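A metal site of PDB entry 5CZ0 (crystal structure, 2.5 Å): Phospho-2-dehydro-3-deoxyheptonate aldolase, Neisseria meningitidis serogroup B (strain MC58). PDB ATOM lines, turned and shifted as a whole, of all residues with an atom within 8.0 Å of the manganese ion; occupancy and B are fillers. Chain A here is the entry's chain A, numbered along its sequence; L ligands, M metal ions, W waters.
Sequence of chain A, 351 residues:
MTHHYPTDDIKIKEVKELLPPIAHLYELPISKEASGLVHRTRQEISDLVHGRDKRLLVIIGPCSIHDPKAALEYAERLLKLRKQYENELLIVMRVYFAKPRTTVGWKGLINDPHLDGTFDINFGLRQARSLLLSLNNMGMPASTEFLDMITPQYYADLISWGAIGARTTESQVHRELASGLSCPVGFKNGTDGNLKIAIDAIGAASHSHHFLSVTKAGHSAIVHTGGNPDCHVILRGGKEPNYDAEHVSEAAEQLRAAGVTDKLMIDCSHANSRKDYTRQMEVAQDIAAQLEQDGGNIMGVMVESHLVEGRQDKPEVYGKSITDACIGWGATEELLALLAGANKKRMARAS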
ATOM      1  N   GLY A  61      10.182   3.980  22.958  1.00  0.00           N
ATOM      2  CA  GLY A  61       9.672   2.920  23.781  1.00  0.00           C
ATOM      3  C   GLY A  61      10.843   2.237  24.430  1.00  0.00           C
ATOM      4  O   GLY A  61      11.962   2.705  24.299  1.00  0.00           O
ATOM      5  N   PRO A  62      10.591   1.154  25.160  1.00  0.00           N
ATOM      6  CA  PRO A  62      11.640   0.441  25.860  1.00  0.00           C
ATOM      7  C   PRO A  62      12.719  -0.075  24.932  1.00  0.00           C
ATOM      8  O   PRO A  62      12.484  -0.263  23.742  1.00  0.00           O
ATOM      9  CB  PRO A  62      10.913  -0.766  26.435  1.00  0.00           C
ATOM     10  CG  PRO A  62       9.488  -0.354  26.539  1.00  0.00           C
ATOM     11  CD  PRO A  62       9.279   0.508  25.330  1.00  0.00           C
ATOM     12  N   CYS A  63      13.909  -0.265  25.477  1.00  0.00           N
ATOM     13  CA  CYS A  63      14.981  -0.951  24.771  1.00  0.00           C
ATOM     14  C   CYS A  63      14.516  -2.385  24.421  1.00  0.00           C
ATOM     15  O   CYS A  63      14.601  -2.809  23.284  1.00  0.00           O
ATOM     16  CB  CYS A  63      16.234  -0.953  25.625  1.00  0.00           C
ATOM     17  SG  CYS A  63      17.551  -2.032  25.005  1.00  0.00           S
ATOM     18  N   SER A  64      13.980  -3.126  25.400  1.00  0.00           N
ATOM     19  CA  SER A  64      13.393  -4.399  25.109  1.00  0.00           C
ATOM     20  C   SER A  64      12.137  -4.696  25.911  1.00  0.00           C
ATOM     21  O   SER A  64      12.005  -4.328  27.085  1.00  0.00           O
ATOM     22  CB  SER A  64      14.391  -5.504  25.372  1.00  0.00           C
ATOM     23  OG  SER A  64      14.810  -5.467  26.736  1.00  0.00           O
ATOM     24  N   ARG A  94       8.475   1.465  20.150  1.00  0.00           N
ATOM     25  CA  ARG A  94       9.586   0.540  19.977  1.00  0.00           C
ATOM     26  C   ARG A  94       9.074  -0.695  20.614  1.00  0.00           C
ATOM     27  O   ARG A  94       8.830  -0.687  21.825  1.00  0.00           O
ATOM     28  CB  ARG A  94      10.836   0.902  20.820  1.00  0.00           C
ATOM     29  CG  ARG A  94      11.931   1.723  20.198  1.00  0.00           C
ATOM     30  CD  ARG A  94      13.068   2.047  21.183  1.00  0.00           C
ATOM     31  NE  ARG A  94      13.850   0.848  21.514  1.00  0.00           N
ATOM     32  CZ  ARG A  94      14.956   0.429  20.882  1.00  0.00           C
ATOM     33  NH1 ARG A  94      15.542   1.120  19.902  1.00  0.00           N
ATOM     34  NH2 ARG A  94      15.485  -0.715  21.269  1.00  0.00           N
ATOM     35  N   TYR A  96      10.759  -4.043  20.580  1.00  0.00           N
ATOM     36  CA  TYR A  96      11.907  -4.877  20.222  1.00  0.00           C
ATOM     37  C   TYR A  96      11.907  -6.174  21.012  1.00  0.00           C
ATOM     38  O   TYR A  96      11.976  -6.178  22.244  1.00  0.00           O
ATOM     39  CB  TYR A  96      13.202  -4.149  20.506  1.00  0.00           C
ATOM     40  CG  TYR A  96      13.529  -3.075  19.508  1.00  0.00           C
ATOM     41  CD1 TYR A  96      12.567  -2.168  19.079  1.00  0.00           C
ATOM     42  CD2 TYR A  96      14.809  -2.949  19.024  1.00  0.00           C
ATOM     43  CE1 TYR A  96      12.885  -1.178  18.155  1.00  0.00           C
ATOM     44  CE2 TYR A  96      15.136  -1.949  18.105  1.00  0.00           C
ATOM     45  CZ  TYR A  96      14.169  -1.077  17.656  1.00  0.00           C
ATOM     46  OH  TYR A  96      14.485  -0.106  16.738  1.00  0.00           O
ATOM     47  N   LYS A  99      17.284  -9.063  20.470  1.00  0.00           N
ATOM     48  CA  LYS A  99      18.371  -8.179  20.937  1.00  0.00           C
ATOM     49  C   LYS A  99      19.732  -8.778  20.568  1.00  0.00           C
ATOM     50  O   LYS A  99      19.926 -10.006  20.675  1.00  0.00           O
ATOM     51  CB  LYS A  99      18.286  -8.003  22.478  1.00  0.00           C
ATOM     52  CG  LYS A  99      16.971  -7.440  22.973  1.00  0.00           C
ATOM     53  CD  LYS A  99      16.517  -6.200  22.210  1.00  0.00           C
ATOM     54  CE  LYS A  99      17.574  -5.088  22.219  1.00  0.00           C
ATOM     55  NZ  LYS A  99      17.112  -3.759  21.746  1.00  0.00           N
ATOM     56  N   PRO A 100      20.675  -7.944  20.176  1.00  0.00           N
ATOM     57  CA  PRO A 100      22.004  -8.452  19.856  1.00  0.00           C
ATOM     58  C   PRO A 100      22.951  -8.200  21.005  1.00  0.00           C
ATOM     59  O   PRO A 100      23.261  -7.060  21.300  1.00  0.00           O
ATOM     60  CB  PRO A 100      22.419  -7.627  18.648  1.00  0.00           C
ATOM     61  CG  PRO A 100      21.365  -6.595  18.433  1.00  0.00           C
ATOM     62  CD  PRO A 100      20.448  -6.603  19.614  1.00  0.00           C
ATOM     63  N   GLU A 145      13.297  -4.491  15.582  1.00  0.00           N
ATOM     64  CA  GLU A 145      14.514  -4.772  14.870  1.00  0.00           C
ATOM     65  C   GLU A 145      14.412  -6.174  14.347  1.00  0.00           C
ATOM     66  O   GLU A 145      14.010  -7.067  15.075  1.00  0.00           O
ATOM     67  CB  GLU A 145      15.751  -4.632  15.737  1.00  0.00           C
ATOM     68  CG  GLU A 145      16.994  -4.873  14.912  1.00  0.00           C
ATOM     69  CD  GLU A 145      18.252  -5.004  15.720  1.00  0.00           C
ATOM     70  OE1 GLU A 145      18.479  -4.177  16.634  1.00  0.00           O
ATOM     71  OE2 GLU A 145      19.038  -5.901  15.383  1.00  0.00           O
ATOM     72  N   LYS A 188      21.456   1.138  10.691  1.00  0.00           N
ATOM     73  CA  LYS A 188      22.308   1.875  11.599  1.00  0.00           C
ATOM     74  C   LYS A 188      23.751   1.907  11.134  1.00  0.00           C
ATOM     75  O   LYS A 188      24.210   0.973  10.504  1.00  0.00           O
ATOM     76  CB  LYS A 188      22.251   1.256  12.967  1.00  0.00           C
ATOM     77  CG  LYS A 188      20.911   1.505  13.605  1.00  0.00           C
ATOM     78  CD  LYS A 188      20.904   1.208  15.070  1.00  0.00           C
ATOM     79  CE  LYS A 188      20.091   2.248  15.807  1.00  0.00           C
ATOM     80  NZ  LYS A 188      20.156   1.841  17.214  1.00  0.00           N
ATOM     81  N   ASP A 267      19.466   8.533  16.405  1.00  0.00           N
ATOM     82  CA  ASP A 267      19.136   7.801  17.618  1.00  0.00           C
ATOM     83  C   ASP A 267      19.701   8.616  18.765  1.00  0.00           C
ATOM     84  O   ASP A 267      20.901   8.860  18.790  1.00  0.00           O
ATOM     85  CB  ASP A 267      19.778   6.405  17.561  1.00  0.00           C
ATOM     86  CG  ASP A 267      19.594   5.572  18.839  1.00  0.00           C
ATOM     87  OD1 ASP A 267      18.883   6.009  19.769  1.00  0.00           O
ATOM     88  OD2 ASP A 267      20.181   4.472  18.914  1.00  0.00           O
ATOM     89  N   SER A 269      20.011   7.472  21.750  1.00  0.00           N
ATOM     90  CA  SER A 269      20.541   6.598  22.789  1.00  0.00           C
ATOM     91  C   SER A 269      21.800   5.867  22.338  1.00  0.00           C
ATOM     92  O   SER A 269      22.513   6.334  21.457  1.00  0.00           O
ATOM     93  CB  SER A 269      19.473   5.603  23.209  1.00  0.00           C
ATOM     94  OG  SER A 269      19.761   5.116  24.493  1.00  0.00           O
ATOM     95  N   HIS A 270      22.099   4.740  22.960  1.00  0.00           N
ATOM     96  CA  HIS A 270      23.277   3.971  22.592  1.00  0.00           C
ATOM     97  C   HIS A 270      24.512   4.889  22.494  1.00  0.00           C
ATOM     98  O   HIS A 270      24.747   5.680  23.433  1.00  0.00           O
ATOM     99  CB  HIS A 270      22.959   3.143  21.348  1.00  0.00           C
ATOM    100  CG  HIS A 270      21.677   2.400  21.486  1.00  0.00           C
ATOM    101  ND1 HIS A 270      20.519   2.775  20.832  1.00  0.00           N
ATOM    102  CD2 HIS A 270      21.328   1.362  22.291  1.00  0.00           C
ATOM    103  CE1 HIS A 270      19.532   1.976  21.208  1.00  0.00           C
ATOM    104  NE2 HIS A 270      19.994   1.126  22.101  1.00  0.00           N
ATOM    105  N   MET A 302      15.121   8.530  17.480  1.00  0.00           N
ATOM    106  CA  MET A 302      14.872   7.331  18.249  1.00  0.00           C
ATOM    107  C   MET A 302      15.137   7.671  19.712  1.00  0.00           C
ATOM    108  O   MET A 302      16.088   8.395  20.008  1.00  0.00           O
ATOM    109  CB  MET A 302      15.774   6.196  17.758  1.00  0.00           C
ATOM    110  CG  MET A 302      15.465   4.819  18.339  1.00  0.00           C
ATOM    111  SD  MET A 302      16.554   3.530  17.657  1.00  0.00           S
ATOM    112  CE  MET A 302      16.284   3.739  15.898  1.00  0.00           C
ATOM    113  N   GLU A 304      15.044   5.725  23.723  1.00  0.00           N
ATOM    114  CA  GLU A 304      14.796   4.637  24.674  1.00  0.00           C
ATOM    115  C   GLU A 304      14.070   5.097  25.994  1.00  0.00           C
ATOM    116  O   GLU A 304      14.653   5.674  26.927  1.00  0.00           O
ATOM    117  CB  GLU A 304      16.085   3.853  24.941  1.00  0.00           C
ATOM    118  CG  GLU A 304      16.499   3.011  23.729  1.00  0.00           C
ATOM    119  CD  GLU A 304      17.718   2.122  23.951  1.00  0.00           C
ATOM    120  OE1 GLU A 304      18.768   2.646  24.382  1.00  0.00           O
ATOM    121  OE2 GLU A 304      17.653   0.903  23.664  1.00  0.00           O
ATOM    122  N   SER A 321      13.459  -1.165  32.506  1.00  0.00           N
ATOM    123  CA  SER A 321      14.280  -1.985  31.541  1.00  0.00           C
ATOM    124  C   SER A 321      15.195  -2.989  32.208  1.00  0.00           C
ATOM    125  O   SER A 321      15.754  -2.687  33.237  1.00  0.00           O
ATOM    126  CB  SER A 321      15.138  -1.063  30.647  1.00  0.00           C
ATOM    127  OG  SER A 321      15.887  -1.794  29.658  1.00  0.00           O
ATOM    128  N   THR A 323      17.401  -4.459  29.922  1.00  0.00           N
ATOM    129  CA  THR A 323      18.527  -4.245  29.046  1.00  0.00           C
ATOM    130  C   THR A 323      19.076  -2.823  29.246  1.00  0.00           C
ATOM    131  O   THR A 323      19.505  -2.461  30.338  1.00  0.00           O
ATOM    132  CB  THR A 323      18.167  -4.589  27.590  1.00  0.00           C
ATOM    133  OG1 THR A 323      16.985  -3.897  27.203  1.00  0.00           O
ATOM    134  CG2 THR A 323      17.945  -6.060  27.443  1.00  0.00           C
ATOM    135  N   ASP A 324      19.097  -1.990  28.223  1.00  0.00           N
ATOM    136  CA  ASP A 324      19.758  -0.697  28.399  1.00  0.00           C
ATOM    137  C   ASP A 324      18.871   0.215  29.237  1.00  0.00           C
ATOM    138  O   ASP A 324      17.662  -0.024  29.386  1.00  0.00           O
ATOM    139  CB  ASP A 324      20.155  -0.040  27.061  1.00  0.00           C
ATOM    140  CG  ASP A 324      20.994  -0.961  26.160  1.00  0.00           C
ATOM    141  OD1 ASP A 324      21.626  -1.898  26.675  1.00  0.00           O
ATOM    142  OD2 ASP A 324      20.954  -0.760  24.933  1.00  0.00           O
ATOM    143  N   ALA A 325      19.481   1.243  29.799  1.00  0.00           N
ATOM    144  CA  ALA A 325      18.780   2.130  30.696  1.00  0.00           C
ATOM    145  C   ALA A 325      17.899   3.023  29.869  1.00  0.00           C
ATOM    146  O   ALA A 325      18.308   3.462  28.824  1.00  0.00           O
ATOM    147  CB  ALA A 325      19.756   2.955  31.500  1.00  0.00           C
ATOM    148  N   CYS A 326      16.682   3.276  30.361  1.00  0.00           N
ATOM    149  CA  CYS A 326      15.730   4.127  29.691  1.00  0.00           C
ATOM    150  C   CYS A 326      15.345   5.339  30.539  1.00  0.00           C
ATOM    151  O   CYS A 326      15.376   5.277  31.772  1.00  0.00           O
ATOM    152  CB  CYS A 326      14.482   3.322  29.384  1.00  0.00           C
ATOM    153  SG  CYS A 326      14.756   1.969  28.214  1.00  0.00           S
HETATM  154  C1  LIG L   1      18.764  -0.957  19.312  1.00  0.00           C
HETATM  155  O1  LIG L   1      18.088  -0.885  20.349  1.00  0.00           O
HETATM  156  O2  LIG L   1      18.357  -0.481  18.228  1.00  0.00           O
HETATM  157  C2  LIG L   1      20.069  -1.598  19.380  1.00  0.00           C
HETATM  158  C3  LIG L   1      20.190  -2.908  19.566  1.00  0.00           C
HETATM  159  O3  LIG L   1      21.240  -0.722  19.278  1.00  0.00           O
HETATM  160  P1  LIG L   1      22.337  -0.717  18.078  1.00  0.00           P
HETATM  161  O4  LIG L   1      23.524  -1.444  18.688  1.00  0.00           O
HETATM  162  O5  LIG L   1      22.561   0.776  17.955  1.00  0.00           O
HETATM  163  O6  LIG L   1      21.690  -1.459  16.918  1.00  0.00           O
HETATM  164 MN    MN M   1      19.102  -0.532  23.669  1.00  0.00          MN
HETATM  165  O   HOH W   1      19.419  -2.251  22.568  1.00  0.00           O
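A ring nitrogen (NE2) of His 270 lies close to an oxygen (O1) of the ligand. An oxygen (O1) of the ligand lies within salt-bridge range of the side-chain amino group (NZ) of Lys 99 (3.3 Å). NH2 of Arg 94 lies within salt-bridge range of O1 of the ligand. An oxygen (O5) of the ligand lies within salt-bridge range of the side-chain amino group (NZ) of Lys 188.
The backbone carbonyl oxygen (O) of Cys 63 sits at hydrogen-bond distance from the side-chain amino group (NZ) of Lys 99 (3.1 Å). The side-chain carboxylate of Glu 304 sits at hydrogen-bond distance from the side-chain hydroxyl of Ser 269, at 2.7 Å. The backbone carbonyl oxygen (O) of Asp 324 is in hydrogen-bond range of the side-chain sulfur (SG) of Cys 326 (3.7 Å). NH2 of Arg 94 sits at hydrogen-bond distance from O of Cys 63 (3.0 Å). OG of Ser 321 is in hydrogen-bond range of O of Asp 324, 2.5 Å away. N of Cys 63 is in hydrogen-bond range of SG of Cys 326 (3.6 Å). The guanidinium group (NH2) of Arg 94 sits close to the side-chain carboxylate (OE2) of Glu 304 (3.6 Å). The side-chain carboxylate (OD2) of Asp 267 sits at hydrogen-bond distance from a ring nitrogen (ND1) of His 270, 2.6 Å away.
The manganese ion is bound by the side-chain carboxylate (OE2) of Glu 304, water W1, the side-chain carboxylate (OD2) of Asp 324, a ring nitrogen (NE2) of His 270 and the side-chain sulfur (SG) of Cys 63. The manganese ion has five donor atoms within binding distance.
Water W1 bridges the side-chain amino group of Lys 99 (2.9 Å) and an oxygen (O1) of the ligand (2.9 Å).
Within 4 Å of the manganese ion: Cys 63, His 270, Glu 304 and Asp 324.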
